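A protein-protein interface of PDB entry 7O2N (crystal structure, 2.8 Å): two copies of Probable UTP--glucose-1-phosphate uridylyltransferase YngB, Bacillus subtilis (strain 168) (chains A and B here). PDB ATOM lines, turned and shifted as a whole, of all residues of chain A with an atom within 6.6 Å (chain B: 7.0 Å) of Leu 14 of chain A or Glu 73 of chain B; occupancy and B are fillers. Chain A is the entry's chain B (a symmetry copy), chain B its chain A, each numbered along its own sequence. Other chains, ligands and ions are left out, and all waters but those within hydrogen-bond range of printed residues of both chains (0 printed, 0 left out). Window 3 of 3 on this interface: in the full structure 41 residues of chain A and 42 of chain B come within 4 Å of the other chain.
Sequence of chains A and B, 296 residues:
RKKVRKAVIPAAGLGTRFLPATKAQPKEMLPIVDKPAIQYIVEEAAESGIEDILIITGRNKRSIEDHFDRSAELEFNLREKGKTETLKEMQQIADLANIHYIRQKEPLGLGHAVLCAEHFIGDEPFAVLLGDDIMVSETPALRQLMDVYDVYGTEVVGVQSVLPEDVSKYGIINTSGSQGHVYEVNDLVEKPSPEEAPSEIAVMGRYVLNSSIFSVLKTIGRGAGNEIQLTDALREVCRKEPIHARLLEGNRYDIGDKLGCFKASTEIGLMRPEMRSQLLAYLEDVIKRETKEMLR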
ATOM      1  N   ALA A  12      15.476  -5.299  -5.101  1.00  0.00           N
ATOM      2  CA  ALA A  12      14.442  -4.634  -4.327  1.00  0.00           C
ATOM      3  C   ALA A  12      13.508  -5.650  -3.680  1.00  0.00           C
ATOM      4  O   ALA A  12      12.683  -5.274  -2.846  1.00  0.00           O
ATOM      5  CB  ALA A  12      13.706  -3.642  -5.179  1.00  0.00           C
ATOM      6  N   GLY A  13      13.682  -6.933  -4.041  1.00  0.00           N
ATOM      7  CA  GLY A  13      12.892  -8.045  -3.514  1.00  0.00           C
ATOM      8  C   GLY A  13      12.829  -8.075  -1.989  1.00  0.00           C
ATOM      9  O   GLY A  13      13.791  -7.754  -1.311  1.00  0.00           O
ATOM     10  N   LEU A  14      11.692  -8.486  -1.448  1.00  0.00           N
ATOM     11  CA  LEU A  14      11.471  -8.542  -0.017  1.00  0.00           C
ATOM     12  C   LEU A  14      11.938  -9.912   0.487  1.00  0.00           C
ATOM     13  O   LEU A  14      11.920 -10.181   1.696  1.00  0.00           O
ATOM     14  CB  LEU A  14       9.961  -8.345   0.170  1.00  0.00           C
ATOM     15  CG  LEU A  14       9.454  -7.755   1.488  1.00  0.00           C
ATOM     16  CD1 LEU A  14       8.539  -6.563   1.238  1.00  0.00           C
ATOM     17  CD2 LEU A  14       8.688  -8.801   2.291  1.00  0.00           C
ATOM     18  N   GLY A  15      12.337 -10.772  -0.473  1.00  0.00           N
ATOM     19  CA  GLY A  15      12.900 -12.091  -0.236  1.00  0.00           C
ATOM     20  C   GLY A  15      12.058 -12.947   0.707  1.00  0.00           C
ATOM     21  O   GLY A  15      12.505 -13.312   1.790  1.00  0.00           O
ATOM     22  N   THR A  16      10.854 -13.315   0.262  1.00  0.00           N
ATOM     23  CA  THR A  16       9.911 -14.038   1.104  1.00  0.00           C
ATOM     24  C   THR A  16      10.265 -15.523   1.200  1.00  0.00           C
ATOM     25  O   THR A  16       9.965 -16.159   2.207  1.00  0.00           O
ATOM     26  CB  THR A  16       8.484 -13.789   0.622  1.00  0.00           C
ATOM     27  OG1 THR A  16       8.599 -13.081  -0.617  1.00  0.00           O
ATOM     28  CG2 THR A  16       7.695 -12.979   1.625  1.00  0.00           C
ATOM     29  N   ARG A  17      10.916 -16.054   0.150  1.00  0.00           N
ATOM     30  CA  ARG A  17      11.264 -17.465   0.062  1.00  0.00           C
ATOM     31  C   ARG A  17      12.202 -17.884   1.195  1.00  0.00           C
ATOM     32  O   ARG A  17      12.486 -19.071   1.351  1.00  0.00           O
ATOM     33  CB  ARG A  17      11.901 -17.784  -1.295  1.00  0.00           C
ATOM     34  CG  ARG A  17      10.974 -17.539  -2.470  1.00  0.00           C
ATOM     35  CD  ARG A  17      11.068 -18.583  -3.570  1.00  0.00           C
ATOM     36  NE  ARG A  17      10.528 -18.081  -4.829  1.00  0.00           N
ATOM     37  CZ  ARG A  17      11.234 -17.408  -5.737  1.00  0.00           C
ATOM     38  NH1 ARG A  17      12.523 -17.172  -5.541  1.00  0.00           N
ATOM     39  NH2 ARG A  17      10.650 -16.976  -6.841  1.00  0.00           N
ATOM     40  N   LEU A  19      12.179 -16.622   4.596  1.00  0.00           N
ATOM     41  CA  LEU A  19      11.773 -16.265   5.943  1.00  0.00           C
ATOM     42  C   LEU A  19      11.989 -17.492   6.824  1.00  0.00           C
ATOM     43  O   LEU A  19      12.019 -18.621   6.329  1.00  0.00           O
ATOM     44  CB  LEU A  19      10.302 -15.820   5.922  1.00  0.00           C
ATOM     45  CG  LEU A  19      10.019 -14.405   5.400  1.00  0.00           C
ATOM     46  CD1 LEU A  19      11.027 -13.925   4.365  1.00  0.00           C
ATOM     47  CD2 LEU A  19       8.620 -14.290   4.824  1.00  0.00           C
ATOM     48  N   THR A  22      15.100 -13.666   6.476  1.00  0.00           N
ATOM     49  CA  THR A  22      15.004 -12.369   5.824  1.00  0.00           C
ATOM     50  C   THR A  22      13.903 -11.490   6.415  1.00  0.00           C
ATOM     51  O   THR A  22      13.632 -10.415   5.893  1.00  0.00           O
ATOM     52  CB  THR A  22      14.758 -12.497   4.323  1.00  0.00           C
ATOM     53  OG1 THR A  22      13.823 -13.566   4.230  1.00  0.00           O
ATOM     54  CG2 THR A  22      16.000 -12.828   3.528  1.00  0.00           C
ATOM     55  N   LYS A  23      13.292 -11.906   7.521  1.00  0.00           N
ATOM     56  CA  LYS A  23      12.289 -11.071   8.157  1.00  0.00           C
ATOM     57  C   LYS A  23      12.801  -9.638   8.315  1.00  0.00           C
ATOM     58  O   LYS A  23      12.098  -8.701   7.980  1.00  0.00           O
ATOM     59  CB  LYS A  23      11.868 -11.669   9.503  1.00  0.00           C
ATOM     60  CG  LYS A  23      10.734 -10.947  10.225  1.00  0.00           C
ATOM     61  CD  LYS A  23      10.621 -11.387  11.669  1.00  0.00           C
ATOM     62  CE  LYS A  23       9.266 -11.195  12.312  1.00  0.00           C
ATOM     63  NZ  LYS A  23       9.065  -9.793  12.752  1.00  0.00           N
ATOM     64  N   GLN A  25      16.145  -8.573   7.438  1.00  0.00           N
ATOM     65  CA  GLN A  25      17.371  -8.286   6.714  1.00  0.00           C
ATOM     66  C   GLN A  25      17.315  -8.824   5.284  1.00  0.00           C
ATOM     67  O   GLN A  25      16.574  -9.742   4.978  1.00  0.00           O
ATOM     68  CB  GLN A  25      18.598  -8.714   7.520  1.00  0.00           C
ATOM     69  CG  GLN A  25      18.764 -10.206   7.697  1.00  0.00           C
ATOM     70  CD  GLN A  25      19.762 -10.462   8.805  1.00  0.00           C
ATOM     71  OE1 GLN A  25      20.405  -9.527   9.342  1.00  0.00           O
ATOM     72  NE2 GLN A  25      19.886 -11.741   9.150  1.00  0.00           N
ATOM     73  N   PRO A  26      18.092  -8.271   4.336  1.00  0.00           N
ATOM     74  CA  PRO A  26      17.880  -8.546   2.922  1.00  0.00           C
ATOM     75  C   PRO A  26      18.363  -9.906   2.446  1.00  0.00           C
ATOM     76  O   PRO A  26      19.376 -10.419   2.912  1.00  0.00           O
ATOM     77  CB  PRO A  26      18.752  -7.497   2.224  1.00  0.00           C
ATOM     78  CG  PRO A  26      19.135  -6.529   3.318  1.00  0.00           C
ATOM     79  CD  PRO A  26      19.206  -7.349   4.575  1.00  0.00           C
ATOM     80  N   LYS A  27      17.632 -10.443   1.471  1.00  0.00           N
ATOM     81  CA  LYS A  27      17.939 -11.684   0.786  1.00  0.00           C
ATOM     82  C   LYS A  27      19.396 -11.648   0.307  1.00  0.00           C
ATOM     83  O   LYS A  27      20.126 -12.631   0.428  1.00  0.00           O
ATOM     84  CB  LYS A  27      16.885 -11.841  -0.317  1.00  0.00           C
ATOM     85  CG  LYS A  27      17.169 -12.847  -1.426  1.00  0.00           C
ATOM     86  CD  LYS A  27      16.805 -12.357  -2.823  1.00  0.00           C
ATOM     87  CE  LYS A  27      15.313 -12.230  -3.076  1.00  0.00           C
ATOM     88  NZ  LYS A  27      14.977 -11.074  -3.944  1.00  0.00           N
ATOM     89  N   GLU A  28      19.837 -10.495  -0.207  1.00  0.00           N
ATOM     90  CA  GLU A  28      21.082 -10.457  -0.960  1.00  0.00           C
ATOM     91  C   GLU A  28      22.297 -10.407  -0.039  1.00  0.00           C
ATOM     92  O   GLU A  28      23.433 -10.539  -0.510  1.00  0.00           O
ATOM     93  CB  GLU A  28      21.086  -9.387  -2.059  1.00  0.00           C
ATOM     94  CG  GLU A  28      20.100  -8.256  -1.850  1.00  0.00           C
ATOM     95  CD  GLU A  28      18.640  -8.473  -2.231  1.00  0.00           C
ATOM     96  OE1 GLU A  28      18.315  -8.456  -3.450  1.00  0.00           O
ATOM     97  OE2 GLU A  28      17.814  -8.629  -1.300  1.00  0.00           O
ATOM     98  N   ARG A  59      13.635  -0.474   0.723  1.00  0.00           N
ATOM     99  CA  ARG A  59      13.689  -0.044   2.110  1.00  0.00           C
ATOM    100  C   ARG A  59      14.403  -1.095   2.958  1.00  0.00           C
ATOM    101  O   ARG A  59      14.358  -2.297   2.679  1.00  0.00           O
ATOM    102  CB  ARG A  59      12.267   0.145   2.643  1.00  0.00           C
ATOM    103  CG  ARG A  59      11.897   1.588   2.933  1.00  0.00           C
ATOM    104  CD  ARG A  59      10.424   1.751   2.612  1.00  0.00           C
ATOM    105  NE  ARG A  59      10.350   1.757   1.154  1.00  0.00           N
ATOM    106  CZ  ARG A  59       9.286   1.417   0.441  1.00  0.00           C
ATOM    107  NH1 ARG A  59       8.183   1.024   1.063  1.00  0.00           N
ATOM    108  NH2 ARG A  59       9.345   1.471  -0.882  1.00  0.00           N
ATOM    109  N   ASN A  60      15.050  -0.603   4.016  1.00  0.00           N
ATOM    110  CA  ASN A  60      15.797  -1.404   4.978  1.00  0.00           C
ATOM    111  C   ASN A  60      16.750  -2.352   4.274  1.00  0.00           C
ATOM    112  O   ASN A  60      16.861  -3.493   4.687  1.00  0.00           O
ATOM    113  CB  ASN A  60      14.912  -2.211   5.924  1.00  0.00           C
ATOM    114  CG  ASN A  60      13.612  -1.515   6.242  1.00  0.00           C
ATOM    115  OD1 ASN A  60      12.690  -1.546   5.435  1.00  0.00           O
ATOM    116  ND2 ASN A  60      13.532  -0.886   7.401  1.00  0.00           N
ATOM    117  N   LYS A  61      17.430  -1.868   3.228  1.00  0.00           N
ATOM    118  CA  LYS A  61      18.530  -2.617   2.655  1.00  0.00           C
ATOM    119  C   LYS A  61      19.852  -1.877   2.869  1.00  0.00           C
ATOM    120  O   LYS A  61      20.748  -1.996   2.036  1.00  0.00           O
ATOM    121  CB  LYS A  61      18.236  -2.950   1.190  1.00  0.00           C
ATOM    122  CG  LYS A  61      16.985  -3.783   1.022  1.00  0.00           C
ATOM    123  CD  LYS A  61      16.940  -4.547  -0.274  1.00  0.00           C
ATOM    124  CE  LYS A  61      15.796  -5.539  -0.330  1.00  0.00           C
ATOM    125  NZ  LYS A  61      16.108  -6.630  -1.279  1.00  0.00           N
ATOM    126  N   PRO A 107       7.284  -1.820  -6.097  1.00  0.00           N
ATOM    127  CA  PRO A 107       7.763  -2.966  -6.878  1.00  0.00           C
ATOM    128  C   PRO A 107       6.919  -3.283  -8.110  1.00  0.00           C
ATOM    129  O   PRO A 107       5.808  -3.785  -7.999  1.00  0.00           O
ATOM    130  CB  PRO A 107       7.669  -4.125  -5.873  1.00  0.00           C
ATOM    131  CG  PRO A 107       6.507  -3.747  -4.977  1.00  0.00           C
ATOM    132  CD  PRO A 107       6.562  -2.235  -4.881  1.00  0.00           C
ATOM    133  N   ARG B  70       6.923  -6.293  14.980  1.00  0.00           N
ATOM    134  CA  ARG B  70       6.041  -6.412  13.834  1.00  0.00           C
ATOM    135  C   ARG B  70       6.670  -5.720  12.625  1.00  0.00           C
ATOM    136  O   ARG B  70       7.126  -4.583  12.721  1.00  0.00           O
ATOM    137  CB  ARG B  70       4.686  -5.775  14.140  1.00  0.00           C
ATOM    138  CG  ARG B  70       3.903  -6.445  15.257  1.00  0.00           C
ATOM    139  CD  ARG B  70       2.422  -6.114  15.129  1.00  0.00           C
ATOM    140  NE  ARG B  70       1.712  -7.160  14.397  1.00  0.00           N
ATOM    141  CZ  ARG B  70       1.494  -8.384  14.864  1.00  0.00           C
ATOM    142  NH1 ARG B  70       1.929  -8.721  16.069  1.00  0.00           N
ATOM    143  NH2 ARG B  70       0.850  -9.268  14.123  1.00  0.00           N
ATOM    144  N   SER B  71       6.691  -6.414  11.484  1.00  0.00           N
ATOM    145  CA  SER B  71       7.272  -5.862  10.268  1.00  0.00           C
ATOM    146  C   SER B  71       6.173  -5.476   9.281  1.00  0.00           C
ATOM    147  O   SER B  71       5.783  -6.291   8.443  1.00  0.00           O
ATOM    148  CB  SER B  71       8.268  -6.823   9.643  1.00  0.00           C
ATOM    149  OG  SER B  71       9.006  -7.528  10.634  1.00  0.00           O
ATOM    150  N   ALA B  72       5.708  -4.220   9.370  1.00  0.00           N
ATOM    151  CA  ALA B  72       4.503  -3.763   8.690  1.00  0.00           C
ATOM    152  C   ALA B  72       4.560  -4.025   7.183  1.00  0.00           C
ATOM    153  O   ALA B  72       3.630  -4.584   6.601  1.00  0.00           O
ATOM    154  CB  ALA B  72       4.268  -2.306   8.990  1.00  0.00           C
ATOM    155  N   GLU B  73       5.662  -3.609   6.556  1.00  0.00           N
ATOM    156  CA  GLU B  73       5.796  -3.693   5.115  1.00  0.00           C
ATOM    157  C   GLU B  73       5.838  -5.158   4.660  1.00  0.00           C
ATOM    158  O   GLU B  73       5.592  -5.470   3.491  1.00  0.00           O
ATOM    159  CB  GLU B  73       7.024  -2.896   4.685  1.00  0.00           C
ATOM    160  CG  GLU B  73       7.342  -3.100   3.219  1.00  0.00           C
ATOM    161  CD  GLU B  73       8.066  -1.998   2.475  1.00  0.00           C
ATOM    162  OE1 GLU B  73       8.463  -0.983   3.110  1.00  0.00           O
ATOM    163  OE2 GLU B  73       8.227  -2.168   1.246  1.00  0.00           O
ATOM    164  N   LEU B  74       6.163  -6.063   5.588  1.00  0.00           N
ATOM    165  CA  LEU B  74       6.245  -7.481   5.274  1.00  0.00           C
ATOM    166  C   LEU B  74       4.866  -8.129   5.441  1.00  0.00           C
ATOM    167  O   LEU B  74       4.424  -8.902   4.568  1.00  0.00           O
ATOM    168  CB  LEU B  74       7.284  -8.127   6.195  1.00  0.00           C
ATOM    169  CG  LEU B  74       7.404  -9.648   6.124  1.00  0.00           C
ATOM    170  CD1 LEU B  74       8.004 -10.105   4.802  1.00  0.00           C
ATOM    171  CD2 LEU B  74       8.193 -10.188   7.302  1.00  0.00           C
ATOM    172  N   GLU B  75       4.222  -7.821   6.584  1.00  0.00           N
ATOM    173  CA  GLU B  75       2.863  -8.244   6.874  1.00  0.00           C
ATOM    174  C   GLU B  75       1.950  -7.867   5.710  1.00  0.00           C
ATOM    175  O   GLU B  75       1.200  -8.710   5.243  1.00  0.00           O
ATOM    176  CB  GLU B  75       2.399  -7.695   8.222  1.00  0.00           C
ATOM    177  CG  GLU B  75       2.107  -8.784   9.229  1.00  0.00           C
ATOM    178  CD  GLU B  75       2.523  -8.438  10.647  1.00  0.00           C
ATOM    179  OE1 GLU B  75       3.734  -8.473  10.917  1.00  0.00           O
ATOM    180  OE2 GLU B  75       1.642  -8.124  11.479  1.00  0.00           O
ATOM    181  N   PHE B  76       2.038  -6.623   5.216  1.00  0.00           N
ATOM    182  CA  PHE B  76       1.291  -6.269   4.021  1.00  0.00           C
ATOM    183  C   PHE B  76       1.571  -7.293   2.925  1.00  0.00           C
ATOM    184  O   PHE B  76       0.658  -7.955   2.436  1.00  0.00           O
ATOM    185  CB  PHE B  76       1.536  -4.836   3.536  1.00  0.00           C
ATOM    186  CG  PHE B  76       0.661  -4.463   2.356  1.00  0.00           C
ATOM    187  CD1 PHE B  76       0.997  -4.858   1.064  1.00  0.00           C
ATOM    188  CD2 PHE B  76      -0.527  -3.756   2.531  1.00  0.00           C
ATOM    189  CE1 PHE B  76       0.185  -4.546  -0.019  1.00  0.00           C
ATOM    190  CE2 PHE B  76      -1.334  -3.439   1.444  1.00  0.00           C
ATOM    191  CZ  PHE B  76      -0.976  -3.831   0.170  1.00  0.00           C
ATOM    192  N   ASN B  77       2.844  -7.452   2.572  1.00  0.00           N
ATOM    193  CA  ASN B  77       3.176  -8.265   1.415  1.00  0.00           C
ATOM    194  C   ASN B  77       2.696  -9.704   1.591  1.00  0.00           C
ATOM    195  O   ASN B  77       2.447 -10.408   0.616  1.00  0.00           O
ATOM    196  CB  ASN B  77       4.669  -8.260   1.113  1.00  0.00           C
ATOM    197  CG  ASN B  77       4.921  -8.687  -0.316  1.00  0.00           C
ATOM    198  OD1 ASN B  77       4.222  -8.245  -1.220  1.00  0.00           O
ATOM    199  ND2 ASN B  77       5.889  -9.564  -0.533  1.00  0.00           N
ATOM    200  N   LEU B  78       2.580 -10.142   2.843  1.00  0.00           N
ATOM    201  CA  LEU B  78       2.243 -11.530   3.091  1.00  0.00           C
ATOM    202  C   LEU B  78       0.730 -11.715   2.994  1.00  0.00           C
ATOM    203  O   LEU B  78       0.267 -12.650   2.334  1.00  0.00           O
ATOM    204  CB  LEU B  78       2.786 -11.945   4.462  1.00  0.00           C
ATOM    205  CG  LEU B  78       4.277 -12.299   4.525  1.00  0.00           C
ATOM    206  CD1 LEU B  78       4.569 -12.935   5.869  1.00  0.00           C
ATOM    207  CD2 LEU B  78       4.731 -13.224   3.389  1.00  0.00           C
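Leu 14 of chain A touches just these residues of chain B: Glu 73 (3.9 Å) and Leu 74 (2.9 Å).
Glu 73 of chain B touches two residues of chain A.
Of the printed residues of chain B, Thr 16 of chain A touches Leu 78 (3.5 Å).
Of the printed residues of chain A, Leu 78 of chain B touches Thr 16 (3.5 Å).
Printed residues of chain B within 4 Å of Lys 23 of chain A: Ser 71 (3.1 Å) and Leu 74 (3.9 Å).
Printed residues of chain A within 4 Å of Ser 71 of chain B: Lys 23 (3.1 Å).
The nearest residue of chain A that does not touch Glu 73 of chain B is Asn 60 of chain A (4.9 Å).
No position is printed for both chains.
Of the 6 pairs that touch across the chains among the printed residues, none has its exchanged pair printed and touching as well.
Printed residues of chain A that touch a printed residue of chain B: Leu 14, Thr 16, Lys 23 and Arg 59.
Hydrophobic or aromatic side chains of chain A that line the printed part of chain B: Leu 14.
Printed residues of chain B that touch a printed residue of chain A: Ser 71, Glu 73, Leu 74 and Leu 78.
Hydrophobic or aromatic side chains of chain B within 4 Å of the printed part of chain A: Leu 74 and Leu 78.
Among the printed residues, 6 pairs touch across the chains.
Among the printed residues, Asp or Glu carboxylates within 4 Å of a Lys or Arg side-chain nitrogen of the other chain: Arg 59 of chain A with Glu 73 of chain B (2.9 Å).
Leu 14 of chain A touches Glu 73 of chain B.
Leu 14 of chain A touches Leu 74 of chain B.
Thr 16 of chain A touches Leu 78 of chain B (CG2 to CD2, 3.5 Å).
CD2 of Leu 74 of chain B touches CG of Lys 23 of chain A, at 3.9 Å.
NZ of Lys 23 of chain A lies within hydrogen-bond range of OG of Ser 71 of chain B, 3.1 Å away.
The guanidinium group of Arg 59 of chain A is in salt-bridge range of the side-chain carboxylate of Glu 73 of chain B (2.9 Å).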
